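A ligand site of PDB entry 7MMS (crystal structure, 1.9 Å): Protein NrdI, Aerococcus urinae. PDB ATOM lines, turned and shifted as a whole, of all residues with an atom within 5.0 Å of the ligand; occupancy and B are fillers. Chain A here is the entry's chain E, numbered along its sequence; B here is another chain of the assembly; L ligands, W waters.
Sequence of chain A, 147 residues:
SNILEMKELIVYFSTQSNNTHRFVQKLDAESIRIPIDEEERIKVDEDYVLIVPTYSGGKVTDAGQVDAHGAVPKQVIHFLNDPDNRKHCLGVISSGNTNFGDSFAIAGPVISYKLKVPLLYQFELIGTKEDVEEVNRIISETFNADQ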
ATOM      1  N   PHE A  13      25.836 -14.721   1.792  1.00  0.00           N
ATOM      2  CA  PHE A  13      25.924 -13.257   1.995  1.00  0.00           C
ATOM      3  C   PHE A  13      24.504 -12.700   2.129  1.00  0.00           C
ATOM      4  O   PHE A  13      23.574 -13.219   1.473  1.00  0.00           O
ATOM      5  CB  PHE A  13      26.684 -12.561   0.871  1.00  0.00           C
ATOM      6  CG  PHE A  13      26.764 -11.066   1.029  1.00  0.00           C
ATOM      7  CD1 PHE A  13      27.697 -10.500   1.879  1.00  0.00           C
ATOM      8  CD2 PHE A  13      25.856 -10.232   0.389  1.00  0.00           C
ATOM      9  CE1 PHE A  13      27.761  -9.120   2.051  1.00  0.00           C
ATOM     10  CE2 PHE A  13      25.908  -8.857   0.582  1.00  0.00           C
ATOM     11  CZ  PHE A  13      26.858  -8.305   1.403  1.00  0.00           C
ATOM     12  N   SER A  14      24.355 -11.679   2.959  1.00  0.00           N
ATOM     13  CA  SER A  14      23.097 -10.919   3.159  1.00  0.00           C
ATOM     14  C   SER A  14      23.459  -9.495   3.586  1.00  0.00           C
ATOM     15  O   SER A  14      24.299  -9.356   4.482  1.00  0.00           O
ATOM     16  CB  SER A  14      22.225 -11.614   4.182  1.00  0.00           C
ATOM     17  OG  SER A  14      20.906 -11.097   4.158  1.00  0.00           O
ATOM     18  N   THR A  15      22.860  -8.487   2.942  1.00  0.00           N
ATOM     19  CA  THR A  15      23.031  -7.058   3.336  1.00  0.00           C
ATOM     20  C   THR A  15      22.260  -6.829   4.635  1.00  0.00           C
ATOM     21  O   THR A  15      21.784  -7.810   5.237  1.00  0.00           O
ATOM     22  CB  THR A  15      22.590  -6.091   2.223  1.00  0.00           C
ATOM     23  OG1 THR A  15      21.167  -6.121   2.153  1.00  0.00           O
ATOM     24  CG2 THR A  15      23.193  -6.412   0.874  1.00  0.00           C
ATOM     25  N   SER A  17      19.360  -5.700   5.002  1.00  0.00           N
ATOM     26  CA  SER A  17      17.926  -6.061   4.825  1.00  0.00           C
ATOM     27  C   SER A  17      17.672  -7.507   5.270  1.00  0.00           C
ATOM     28  O   SER A  17      16.522  -7.819   5.625  1.00  0.00           O
ATOM     29  CB  SER A  17      17.443  -5.802   3.403  1.00  0.00           C
ATOM     30  OG  SER A  17      18.395  -6.198   2.426  1.00  0.00           O
ATOM     31  N   ASN A  18      18.702  -8.361   5.264  1.00  0.00           N
ATOM     32  CA  ASN A  18      18.708  -9.699   5.912  1.00  0.00           C
ATOM     33  C   ASN A  18      17.670 -10.633   5.276  1.00  0.00           C
ATOM     34  O   ASN A  18      17.220 -11.574   5.980  1.00  0.00           O
ATOM     35  CB  ASN A  18      18.477  -9.572   7.429  1.00  0.00           C
ATOM     36  CG  ASN A  18      19.731  -9.218   8.193  1.00  0.00           C
ATOM     37  OD1 ASN A  18      20.782  -9.814   7.999  1.00  0.00           O
ATOM     38  ND2 ASN A  18      19.627  -8.243   9.086  1.00  0.00           N
ATOM     39  N   ASN A  19      17.309 -10.436   4.002  1.00  0.00           N
ATOM     40  CA  ASN A  19      16.362 -11.328   3.267  1.00  0.00           C
ATOM     41  C   ASN A  19      17.007 -12.707   3.093  1.00  0.00           C
ATOM     42  O   ASN A  19      16.343 -13.725   3.406  1.00  0.00           O
ATOM     43  CB  ASN A  19      15.965 -10.781   1.896  1.00  0.00           C
ATOM     44  CG  ASN A  19      15.042  -9.577   1.948  1.00  0.00           C
ATOM     45  OD1 ASN A  19      14.577  -9.174   3.016  1.00  0.00           O
ATOM     46  ND2 ASN A  19      14.748  -9.006   0.793  1.00  0.00           N
ATOM     47  N   THR A  20      18.254 -12.751   2.614  1.00  0.00           N
ATOM     48  CA  THR A  20      18.998 -14.007   2.331  1.00  0.00           C
ATOM     49  C   THR A  20      19.302 -14.702   3.666  1.00  0.00           C
ATOM     50  O   THR A  20      19.162 -15.939   3.732  1.00  0.00           O
ATOM     51  CB  THR A  20      20.248 -13.757   1.486  1.00  0.00           C
ATOM     52  OG1 THR A  20      19.882 -12.944   0.372  1.00  0.00           O
ATOM     53  CG2 THR A  20      20.875 -15.043   0.978  1.00  0.00           C
ATOM     54  N   HIS A  21      19.687 -13.928   4.689  1.00  0.00           N
ATOM     55  CA  HIS A  21      19.916 -14.419   6.075  1.00  0.00           C
ATOM     56  C   HIS A  21      18.697 -15.214   6.532  1.00  0.00           C
ATOM     57  O   HIS A  21      18.880 -16.375   6.946  1.00  0.00           O
ATOM     58  CB  HIS A  21      20.245 -13.258   7.021  1.00  0.00           C
ATOM     59  CG  HIS A  21      20.256 -13.648   8.461  1.00  0.00           C
ATOM     60  ND1 HIS A  21      21.294 -14.366   9.027  1.00  0.00           N
ATOM     61  CD2 HIS A  21      19.371 -13.425   9.455  1.00  0.00           C
ATOM     62  CE1 HIS A  21      21.037 -14.582  10.306  1.00  0.00           C
ATOM     63  NE2 HIS A  21      19.862 -14.010  10.595  1.00  0.00           N
ATOM     64  N   PRO A  53      22.473 -12.900  -2.801  1.00  0.00           N
ATOM     65  CA  PRO A  53      21.562 -12.035  -3.557  1.00  0.00           C
ATOM     66  C   PRO A  53      22.259 -11.256  -4.692  1.00  0.00           C
ATOM     67  O   PRO A  53      23.475 -11.195  -4.697  1.00  0.00           O
ATOM     68  CB  PRO A  53      21.073 -11.065  -2.477  1.00  0.00           C
ATOM     69  CG  PRO A  53      22.288 -10.886  -1.593  1.00  0.00           C
ATOM     70  CD  PRO A  53      22.950 -12.250  -1.569  1.00  0.00           C
ATOM     71  N   THR A  54      21.467 -10.677  -5.586  1.00  0.00           N
ATOM     72  CA  THR A  54      21.933  -9.907  -6.784  1.00  0.00           C
ATOM     73  C   THR A  54      21.703  -8.411  -6.529  1.00  0.00           C
ATOM     74  O   THR A  54      20.627  -8.075  -6.017  1.00  0.00           O
ATOM     75  CB  THR A  54      21.208 -10.385  -8.047  1.00  0.00           C
ATOM     76  OG1 THR A  54      21.452 -11.787  -8.171  1.00  0.00           O
ATOM     77  CG2 THR A  54      21.673  -9.665  -9.294  1.00  0.00           C
ATOM     78  N   TYR A  55      22.658  -7.563  -6.926  1.00  0.00           N
ATOM     79  CA  TYR A  55      22.628  -6.095  -6.670  1.00  0.00           C
ATOM     80  C   TYR A  55      23.150  -5.303  -7.876  1.00  0.00           C
ATOM     81  O   TYR A  55      23.743  -4.229  -7.664  1.00  0.00           O
ATOM     82  CB  TYR A  55      23.390  -5.795  -5.384  1.00  0.00           C
ATOM     83  CG  TYR A  55      22.556  -5.974  -4.143  1.00  0.00           C
ATOM     84  CD1 TYR A  55      21.683  -4.981  -3.737  1.00  0.00           C
ATOM     85  CD2 TYR A  55      22.612  -7.139  -3.398  1.00  0.00           C
ATOM     86  CE1 TYR A  55      20.890  -5.127  -2.613  1.00  0.00           C
ATOM     87  CE2 TYR A  55      21.821  -7.301  -2.259  1.00  0.00           C
ATOM     88  CZ  TYR A  55      20.960  -6.302  -1.873  1.00  0.00           C
ATOM     89  OH  TYR A  55      20.185  -6.441  -0.757  1.00  0.00           O
ATOM     90  N   SER A  56      22.916  -5.783  -9.109  1.00  0.00           N
ATOM     91  CA  SER A  56      23.246  -5.047 -10.358  1.00  0.00           C
ATOM     92  C   SER A  56      22.276  -3.867 -10.522  1.00  0.00           C
ATOM     93  O   SER A  56      22.728  -2.777 -10.880  1.00  0.00           O
ATOM     94  CB  SER A  56      23.231  -5.945 -11.568  1.00  0.00           C
ATOM     95  OG  SER A  56      21.947  -6.536 -11.755  1.00  0.00           O
ATOM     96  N   GLY A  57      20.978  -4.100 -10.275  1.00  0.00           N
ATOM     97  CA  GLY A  57      19.939  -3.065 -10.196  1.00  0.00           C
ATOM     98  C   GLY A  57      19.207  -2.857 -11.510  1.00  0.00           C
ATOM     99  O   GLY A  57      18.619  -1.773 -11.693  1.00  0.00           O
ATOM    100  N   GLY A  58      19.271  -3.854 -12.408  1.00  0.00           N
ATOM    101  CA  GLY A  58      18.493  -3.897 -13.670  1.00  0.00           C
ATOM    102  C   GLY A  58      19.032  -2.934 -14.721  1.00  0.00           C
ATOM    103  O   GLY A  58      18.257  -2.613 -15.639  1.00  0.00           O
ATOM    104  N   SER A  95      19.600 -15.238  -5.416  1.00  0.00           N
ATOM    105  CA  SER A  95      18.267 -14.658  -5.135  1.00  0.00           C
ATOM    106  C   SER A  95      18.183 -13.270  -5.749  1.00  0.00           C
ATOM    107  O   SER A  95      19.209 -12.739  -6.210  1.00  0.00           O
ATOM    108  CB  SER A  95      17.967 -14.631  -3.660  1.00  0.00           C
ATOM    109  OG  SER A  95      18.847 -13.738  -2.998  1.00  0.00           O
ATOM    110  N   GLY A  96      16.981 -12.704  -5.723  1.00  0.00           N
ATOM    111  CA  GLY A  96      16.677 -11.357  -6.211  1.00  0.00           C
ATOM    112  C   GLY A  96      15.186 -11.152  -6.319  1.00  0.00           C
ATOM    113  O   GLY A  96      14.466 -11.569  -5.376  1.00  0.00           O
ATOM    114  N   ASN A  97      14.739 -10.591  -7.435  1.00  0.00           N
ATOM    115  CA  ASN A  97      13.323 -10.225  -7.675  1.00  0.00           C
ATOM    116  C   ASN A  97      13.094 -10.219  -9.184  1.00  0.00           C
ATOM    117  O   ASN A  97      13.868  -9.556  -9.892  1.00  0.00           O
ATOM    118  CB  ASN A  97      12.983  -8.893  -7.016  1.00  0.00           C
ATOM    119  CG  ASN A  97      11.491  -8.669  -6.858  1.00  0.00           C
ATOM    120  OD1 ASN A  97      10.754  -8.801  -7.832  1.00  0.00           O
ATOM    121  ND2 ASN A  97      11.053  -8.318  -5.667  1.00  0.00           N
ATOM    122  N   PHE A 100      13.194  -7.282 -11.806  1.00  0.00           N
ATOM    123  CA  PHE A 100      14.461  -6.805 -12.439  1.00  0.00           C
ATOM    124  C   PHE A 100      14.648  -7.445 -13.823  1.00  0.00           C
ATOM    125  O   PHE A 100      15.662  -7.140 -14.483  1.00  0.00           O
ATOM    126  CB  PHE A 100      15.663  -7.067 -11.524  1.00  0.00           C
ATOM    127  CG  PHE A 100      15.775  -6.097 -10.373  1.00  0.00           C
ATOM    128  CD1 PHE A 100      16.293  -4.826 -10.557  1.00  0.00           C
ATOM    129  CD2 PHE A 100      15.328  -6.454  -9.108  1.00  0.00           C
ATOM    130  CE1 PHE A 100      16.377  -3.935  -9.495  1.00  0.00           C
ATOM    131  CE2 PHE A 100      15.412  -5.564  -8.046  1.00  0.00           C
ATOM    132  CZ  PHE A 100      15.944  -4.309  -8.242  1.00  0.00           C
ATOM    133  N   SER A 103      17.838  -9.057 -15.504  1.00  0.00           N
ATOM    134  CA  SER A 103      18.849  -8.988 -14.411  1.00  0.00           C
ATOM    135  C   SER A 103      18.427  -9.832 -13.209  1.00  0.00           C
ATOM    136  O   SER A 103      19.162  -9.810 -12.211  1.00  0.00           O
ATOM    137  CB  SER A 103      19.101  -7.551 -14.011  1.00  0.00           C
ATOM    138  OG  SER A 103      19.576  -6.799 -15.120  1.00  0.00           O
ATOM    139  N   PHE A 104      17.314 -10.578 -13.283  1.00  0.00           N
ATOM    140  CA  PHE A 104      16.807 -11.397 -12.150  1.00  0.00           C
ATOM    141  C   PHE A 104      17.862 -12.425 -11.741  1.00  0.00           C
ATOM    142  O   PHE A 104      18.231 -13.277 -12.571  1.00  0.00           O
ATOM    143  CB  PHE A 104      15.480 -12.086 -12.480  1.00  0.00           C
ATOM    144  CG  PHE A 104      15.128 -13.176 -11.499  1.00  0.00           C
ATOM    145  CD1 PHE A 104      15.034 -12.894 -10.139  1.00  0.00           C
ATOM    146  CD2 PHE A 104      14.945 -14.486 -11.913  1.00  0.00           C
ATOM    147  CE1 PHE A 104      14.740 -13.895  -9.233  1.00  0.00           C
ATOM    148  CE2 PHE A 104      14.643 -15.484 -10.996  1.00  0.00           C
ATOM    149  CZ  PHE A 104      14.542 -15.187  -9.665  1.00  0.00           C
ATOM    150  N   ALA A 105      18.328 -12.342 -10.491  1.00  0.00           N
ATOM    151  CA  ALA A 105      19.167 -13.345  -9.796  1.00  0.00           C
ATOM    152  C   ALA A 105      20.466 -13.636 -10.565  1.00  0.00           C
ATOM    153  O   ALA A 105      21.016 -14.736 -10.382  1.00  0.00           O
ATOM    154  CB  ALA A 105      18.368 -14.606  -9.580  1.00  0.00           C
ATOM    155  N   LEU A 125      13.677 -12.994  -2.445  1.00  0.00           N
ATOM    156  CA  LEU A 125      13.464 -12.352  -1.120  1.00  0.00           C
ATOM    157  C   LEU A 125      13.756 -13.392  -0.020  1.00  0.00           C
ATOM    158  O   LEU A 125      14.872 -13.931  -0.030  1.00  0.00           O
ATOM    159  CB  LEU A 125      12.039 -11.791  -1.075  1.00  0.00           C
ATOM    160  CG  LEU A 125      11.678 -10.852  -2.216  1.00  0.00           C
ATOM    161  CD1 LEU A 125      10.208 -10.467  -2.179  1.00  0.00           C
ATOM    162  CD2 LEU A 125      12.554  -9.610  -2.187  1.00  0.00           C
ATOM    163  N   LYS B  41      22.455   1.239   3.565  1.00  0.00           N
ATOM    164  CA  LYS B  41      21.341   0.772   2.687  1.00  0.00           C
ATOM    165  C   LYS B  41      20.719   1.975   1.960  1.00  0.00           C
ATOM    166  O   LYS B  41      20.363   1.809   0.781  1.00  0.00           O
ATOM    167  CB  LYS B  41      20.300  -0.017   3.492  1.00  0.00           C
ATOM    168  CG  LYS B  41      19.131  -0.557   2.687  1.00  0.00           C
ATOM    169  CD  LYS B  41      19.518  -1.518   1.570  1.00  0.00           C
ATOM    170  CE  LYS B  41      20.036  -2.843   2.064  1.00  0.00           C
ATOM    171  NZ  LYS B  41      20.135  -3.835   0.977  1.00  0.00           N
ATOM    172  N   GLU B  44      23.032   2.860  -0.980  1.00  0.00           N
ATOM    173  CA  GLU B  44      22.724   1.744  -1.915  1.00  0.00           C
ATOM    174  C   GLU B  44      21.513   2.135  -2.776  1.00  0.00           C
ATOM    175  O   GLU B  44      21.625   2.148  -4.021  1.00  0.00           O
ATOM    176  CB  GLU B  44      22.421   0.487  -1.092  1.00  0.00           C
ATOM    177  CG  GLU B  44      22.947  -0.818  -1.667  1.00  0.00           C
ATOM    178  CD  GLU B  44      22.953  -1.933  -0.633  1.00  0.00           C
ATOM    179  OE1 GLU B  44      23.696  -1.809   0.377  1.00  0.00           O
ATOM    180  OE2 GLU B  44      22.195  -2.899  -0.797  1.00  0.00           O
ATOM    181  N   VAL B  45      20.390   2.459  -2.138  1.00  0.00           N
ATOM    182  CA  VAL B  45      19.080   2.699  -2.805  1.00  0.00           C
ATOM    183  C   VAL B  45      19.161   4.026  -3.585  1.00  0.00           C
ATOM    184  O   VAL B  45      18.739   4.024  -4.760  1.00  0.00           O
ATOM    185  CB  VAL B  45      17.916   2.683  -1.798  1.00  0.00           C
ATOM    186  CG1 VAL B  45      16.622   3.205  -2.394  1.00  0.00           C
ATOM    187  CG2 VAL B  45      17.706   1.283  -1.229  1.00  0.00           C
ATOM    188  N   ARG B  48      21.181   3.673  -6.856  1.00  0.00           N
ATOM    189  CA  ARG B  48      20.494   2.843  -7.879  1.00  0.00           C
ATOM    190  C   ARG B  48      19.354   3.634  -8.533  1.00  0.00           C
ATOM    191  O   ARG B  48      19.298   3.681  -9.784  1.00  0.00           O
ATOM    192  CB  ARG B  48      19.995   1.512  -7.295  1.00  0.00           C
ATOM    193  CG  ARG B  48      19.391   0.569  -8.318  1.00  0.00           C
ATOM    194  CD  ARG B  48      20.110   0.535  -9.658  1.00  0.00           C
ATOM    195  NE  ARG B  48      21.565   0.437  -9.530  1.00  0.00           N
ATOM    196  CZ  ARG B  48      22.440   0.843 -10.447  1.00  0.00           C
ATOM    197  NH1 ARG B  48      22.042   1.373 -11.588  1.00  0.00           N
ATOM    198  NH2 ARG B  48      23.740   0.715 -10.219  1.00  0.00           N
ATOM    199  N   ILE B 217      12.095  -1.480  -6.225  1.00  0.00           N
ATOM    200  CA  ILE B 217      12.967  -0.805  -5.216  1.00  0.00           C
ATOM    201  C   ILE B 217      12.076  -0.021  -4.232  1.00  0.00           C
ATOM    202  O   ILE B 217      12.367  -0.065  -3.027  1.00  0.00           O
ATOM    203  CB  ILE B 217      14.036   0.078  -5.888  1.00  0.00           C
ATOM    204  CG1 ILE B 217      15.019  -0.799  -6.665  1.00  0.00           C
ATOM    205  CG2 ILE B 217      14.730   0.955  -4.856  1.00  0.00           C
ATOM    206  CD1 ILE B 217      16.194  -0.043  -7.239  1.00  0.00           C
ATOM    207  N   PHE B 220      10.563  -2.562  -1.839  1.00  0.00           N
ATOM    208  CA  PHE B 220      11.671  -3.060  -0.998  1.00  0.00           C
ATOM    209  C   PHE B 220      11.966  -2.039   0.117  1.00  0.00           C
ATOM    210  O   PHE B 220      12.009  -2.435   1.293  1.00  0.00           O
ATOM    211  CB  PHE B 220      12.961  -3.300  -1.791  1.00  0.00           C
ATOM    212  CG  PHE B 220      14.172  -3.291  -0.891  1.00  0.00           C
ATOM    213  CD1 PHE B 220      14.465  -4.391  -0.099  1.00  0.00           C
ATOM    214  CD2 PHE B 220      14.950  -2.162  -0.763  1.00  0.00           C
ATOM    215  CE1 PHE B 220      15.538  -4.372   0.761  1.00  0.00           C
ATOM    216  CE2 PHE B 220      16.037  -2.138   0.107  1.00  0.00           C
ATOM    217  CZ  PHE B 220      16.329  -3.244   0.862  1.00  0.00           C
HETATM  218  C1  LIG L   1      18.140  -5.427  -5.729  1.00  0.00           C
HETATM  219  N1  LIG L   1      17.665  -6.728  -6.053  1.00  0.00           N
HETATM  220  C2  LIG L   1      17.963  -7.297  -7.296  1.00  0.00           C
HETATM  221  N2  LIG L   1      17.395  -8.486  -7.676  1.00  0.00           N
HETATM  222  C3  LIG L   1      17.650  -9.066  -8.893  1.00  0.00           C
HETATM  223  O1  LIG L   1      17.137 -10.117  -9.198  1.00  0.00           O
HETATM  224  N3  LIG L   1      18.520  -8.401  -9.730  1.00  0.00           N
HETATM  225  C4  LIG L   1      19.137  -7.194  -9.438  1.00  0.00           C
HETATM  226  O2  LIG L   1      19.890  -6.689 -10.270  1.00  0.00           O
HETATM  227  C5  LIG L   1      18.844  -6.617  -8.176  1.00  0.00           C
HETATM  228  N4  LIG L   1      19.414  -5.437  -7.773  1.00  0.00           N
HETATM  229  C6  LIG L   1      19.008  -4.789  -6.624  1.00  0.00           C
HETATM  230  C7  LIG L   1      19.478  -3.511  -6.334  1.00  0.00           C
HETATM  231  C8  LIG L   1      19.090  -2.855  -5.193  1.00  0.00           C
HETATM  232  C9  LIG L   1      19.616  -1.470  -4.911  1.00  0.00           C
HETATM  233  C10 LIG L   1      18.186  -3.508  -4.284  1.00  0.00           C
HETATM  234  C11 LIG L   1      17.727  -2.829  -3.011  1.00  0.00           C
HETATM  235  C12 LIG L   1      17.734  -4.765  -4.567  1.00  0.00           C
HETATM  236  C13 LIG L   1      16.791  -7.450  -5.089  1.00  0.00           C
HETATM  237  C14 LIG L   1      17.571  -8.096  -3.958  1.00  0.00           C
HETATM  238  O3  LIG L   1      18.551  -9.009  -4.472  1.00  0.00           O
HETATM  239  C15 LIG L   1      16.600  -8.822  -3.032  1.00  0.00           C
HETATM  240  O4  LIG L   1      15.791  -7.854  -2.360  1.00  0.00           O
HETATM  241  C16 LIG L   1      17.263  -9.720  -1.988  1.00  0.00           C
HETATM  242  O5  LIG L   1      16.241 -10.463  -1.314  1.00  0.00           O
HETATM  243  C17 LIG L   1      18.073  -8.948  -0.977  1.00  0.00           C
HETATM  244  O6  LIG L   1      18.821  -9.888  -0.160  1.00  0.00           O
HETATM  245  P1  LIG L   1      19.492  -9.393   1.214  1.00  0.00           P
HETATM  246  O7  LIG L   1      18.400  -8.776   2.053  1.00  0.00           O
HETATM  247  O8  LIG L   1      20.566  -8.387   0.843  1.00  0.00           O
HETATM  248  O9  LIG L   1      20.050 -10.659   1.833  1.00  0.00           O
HETATM  249  O   HOH W   1      17.519  -5.602  -1.120  1.00  0.00           O
HETATM  250  O   HOH W   2      17.274 -13.017  -0.818  1.00  0.00           O
HETATM  251  O   HOH W   3      13.435  -6.855  -3.988  1.00  0.00           O
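An oxygen (O8) of the ligand lies within hydrogen-bond range of the side-chain hydroxyl (OH) of Tyr 55 (2.5 Å).
ND2 of Asn 19 lies within hydrogen-bond range of O5 of the ligand (3.0 Å).
A nitrogen (N3) of the ligand is in hydrogen-bond range of the backbone carbonyl oxygen of Ser 103 (2.9 Å).
The backbone NH of Asn 97 sits at hydrogen-bond distance from an oxygen (O1) of the ligand (3.0 Å).
The backbone NH (N) of Ser 56 sits at hydrogen-bond distance from an oxygen (O2) of the ligand (3.4 Å).
OG of Ser 56 is in hydrogen-bond range of O2 of the ligand.
N of Asn 18 is in hydrogen-bond range of O7 of the ligand.
N of Gly 57 lies within hydrogen-bond range of O2 of the ligand (2.8 Å).
OG of Ser 14 lies within hydrogen-bond range of O9 of the ligand (2.5 Å).
OG1 of Thr 20 is in hydrogen-bond range of O9 of the ligand, 2.7 Å away.
The backbone NH (N) of Thr 15 lies within hydrogen-bond range of an oxygen (O8) of the ligand, at 3.1 Å.
An oxygen (O7) of the ligand lies within hydrogen-bond range of the side-chain hydroxyl (OG) of Ser 17, at 2.6 Å.
The side-chain hydroxyl (OG1) of Thr 15 sits at hydrogen-bond distance from an oxygen (O8) of the ligand (2.7 Å).
The backbone carbonyl oxygen of Thr 54 sits at hydrogen-bond distance from an oxygen (O3) of the ligand (2.8 Å).
An oxygen (O1) of the ligand lies within hydrogen-bond range of the backbone NH (N) of Ala 105 (2.8 Å).
N of Asn 19 sits at hydrogen-bond distance from O7 of the ligand, 2.8 Å away.
O9 of the ligand sits at hydrogen-bond distance from N of Thr 20, at 2.9 Å.
The backbone carbonyl oxygen (O) of Ser 95 is in hydrogen-bond range of the backbone NH (N) of Thr 54 (3.1 Å).
OG of Ser 14 sits at hydrogen-bond distance from N of Thr 20 (3.5 Å).
OG of Ser 14 sits at hydrogen-bond distance from N of His 21 (3.1 Å).
The side-chain hydroxyl (OG) of Ser 17 is in hydrogen-bond range of the side-chain amino group (NZ) of Lys 41 of chain B (3.3 Å).
The side-chain amino group (NZ) of Lys 41 of chain B lies within hydrogen-bond range of the side-chain hydroxyl (OG1) of Thr 15, at 2.8 Å.
OH of Tyr 55 is in hydrogen-bond range of OG1 of Thr 15, 3.1 Å away.
The side-chain amino group (NZ) of Lys 41 of chain B is in hydrogen-bond range of the side-chain hydroxyl (OH) of Tyr 55 (3.1 Å).
OG1 of Thr 15 sits at hydrogen-bond distance from OG of Ser 17, at 2.8 Å.
Merely in contact with the ligand: Phe 100 (3.2 Å), Phe 104 (3.2 Å), Gly 96 (3.3 Å), Leu 125 (3.4 Å), Pro 53 (3.4 Å), Gly 58 (3.6 Å), Phe 220 of chain B (3.6 Å) and Arg 48 of chain B (3.8 Å).
Hydrophobic or aromatic side chains within 4 Å of the ligand: Pro 53, Tyr 55, Phe 100, Phe 104, Leu 125 and Phe 220 of chain B.
Within 4 Å of the ligand: Ser 14, Thr 15, Ser 17, Asn 18, Asn 19, Thr 20, Pro 53, Thr 54, Tyr 55, Ser 56, Gly 57, Gly 58, Gly 96, Asn 97, Phe 100, Ser 103, Phe 104, Ala 105, Leu 125, Arg 48 of chain B and Phe 220 of chain B.
Water W2 lies within hydrogen-bond range of O of Leu 125, OG of Ser 95, O5 of the ligand and OG1 of Thr 20.
Water W3 bridges O4 of the ligand and ND2 of Asn 97.
Water W1 lies within hydrogen-bond range of OH of Tyr 55 (2.8 Å) and O4 of the ligand (3.1 Å).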
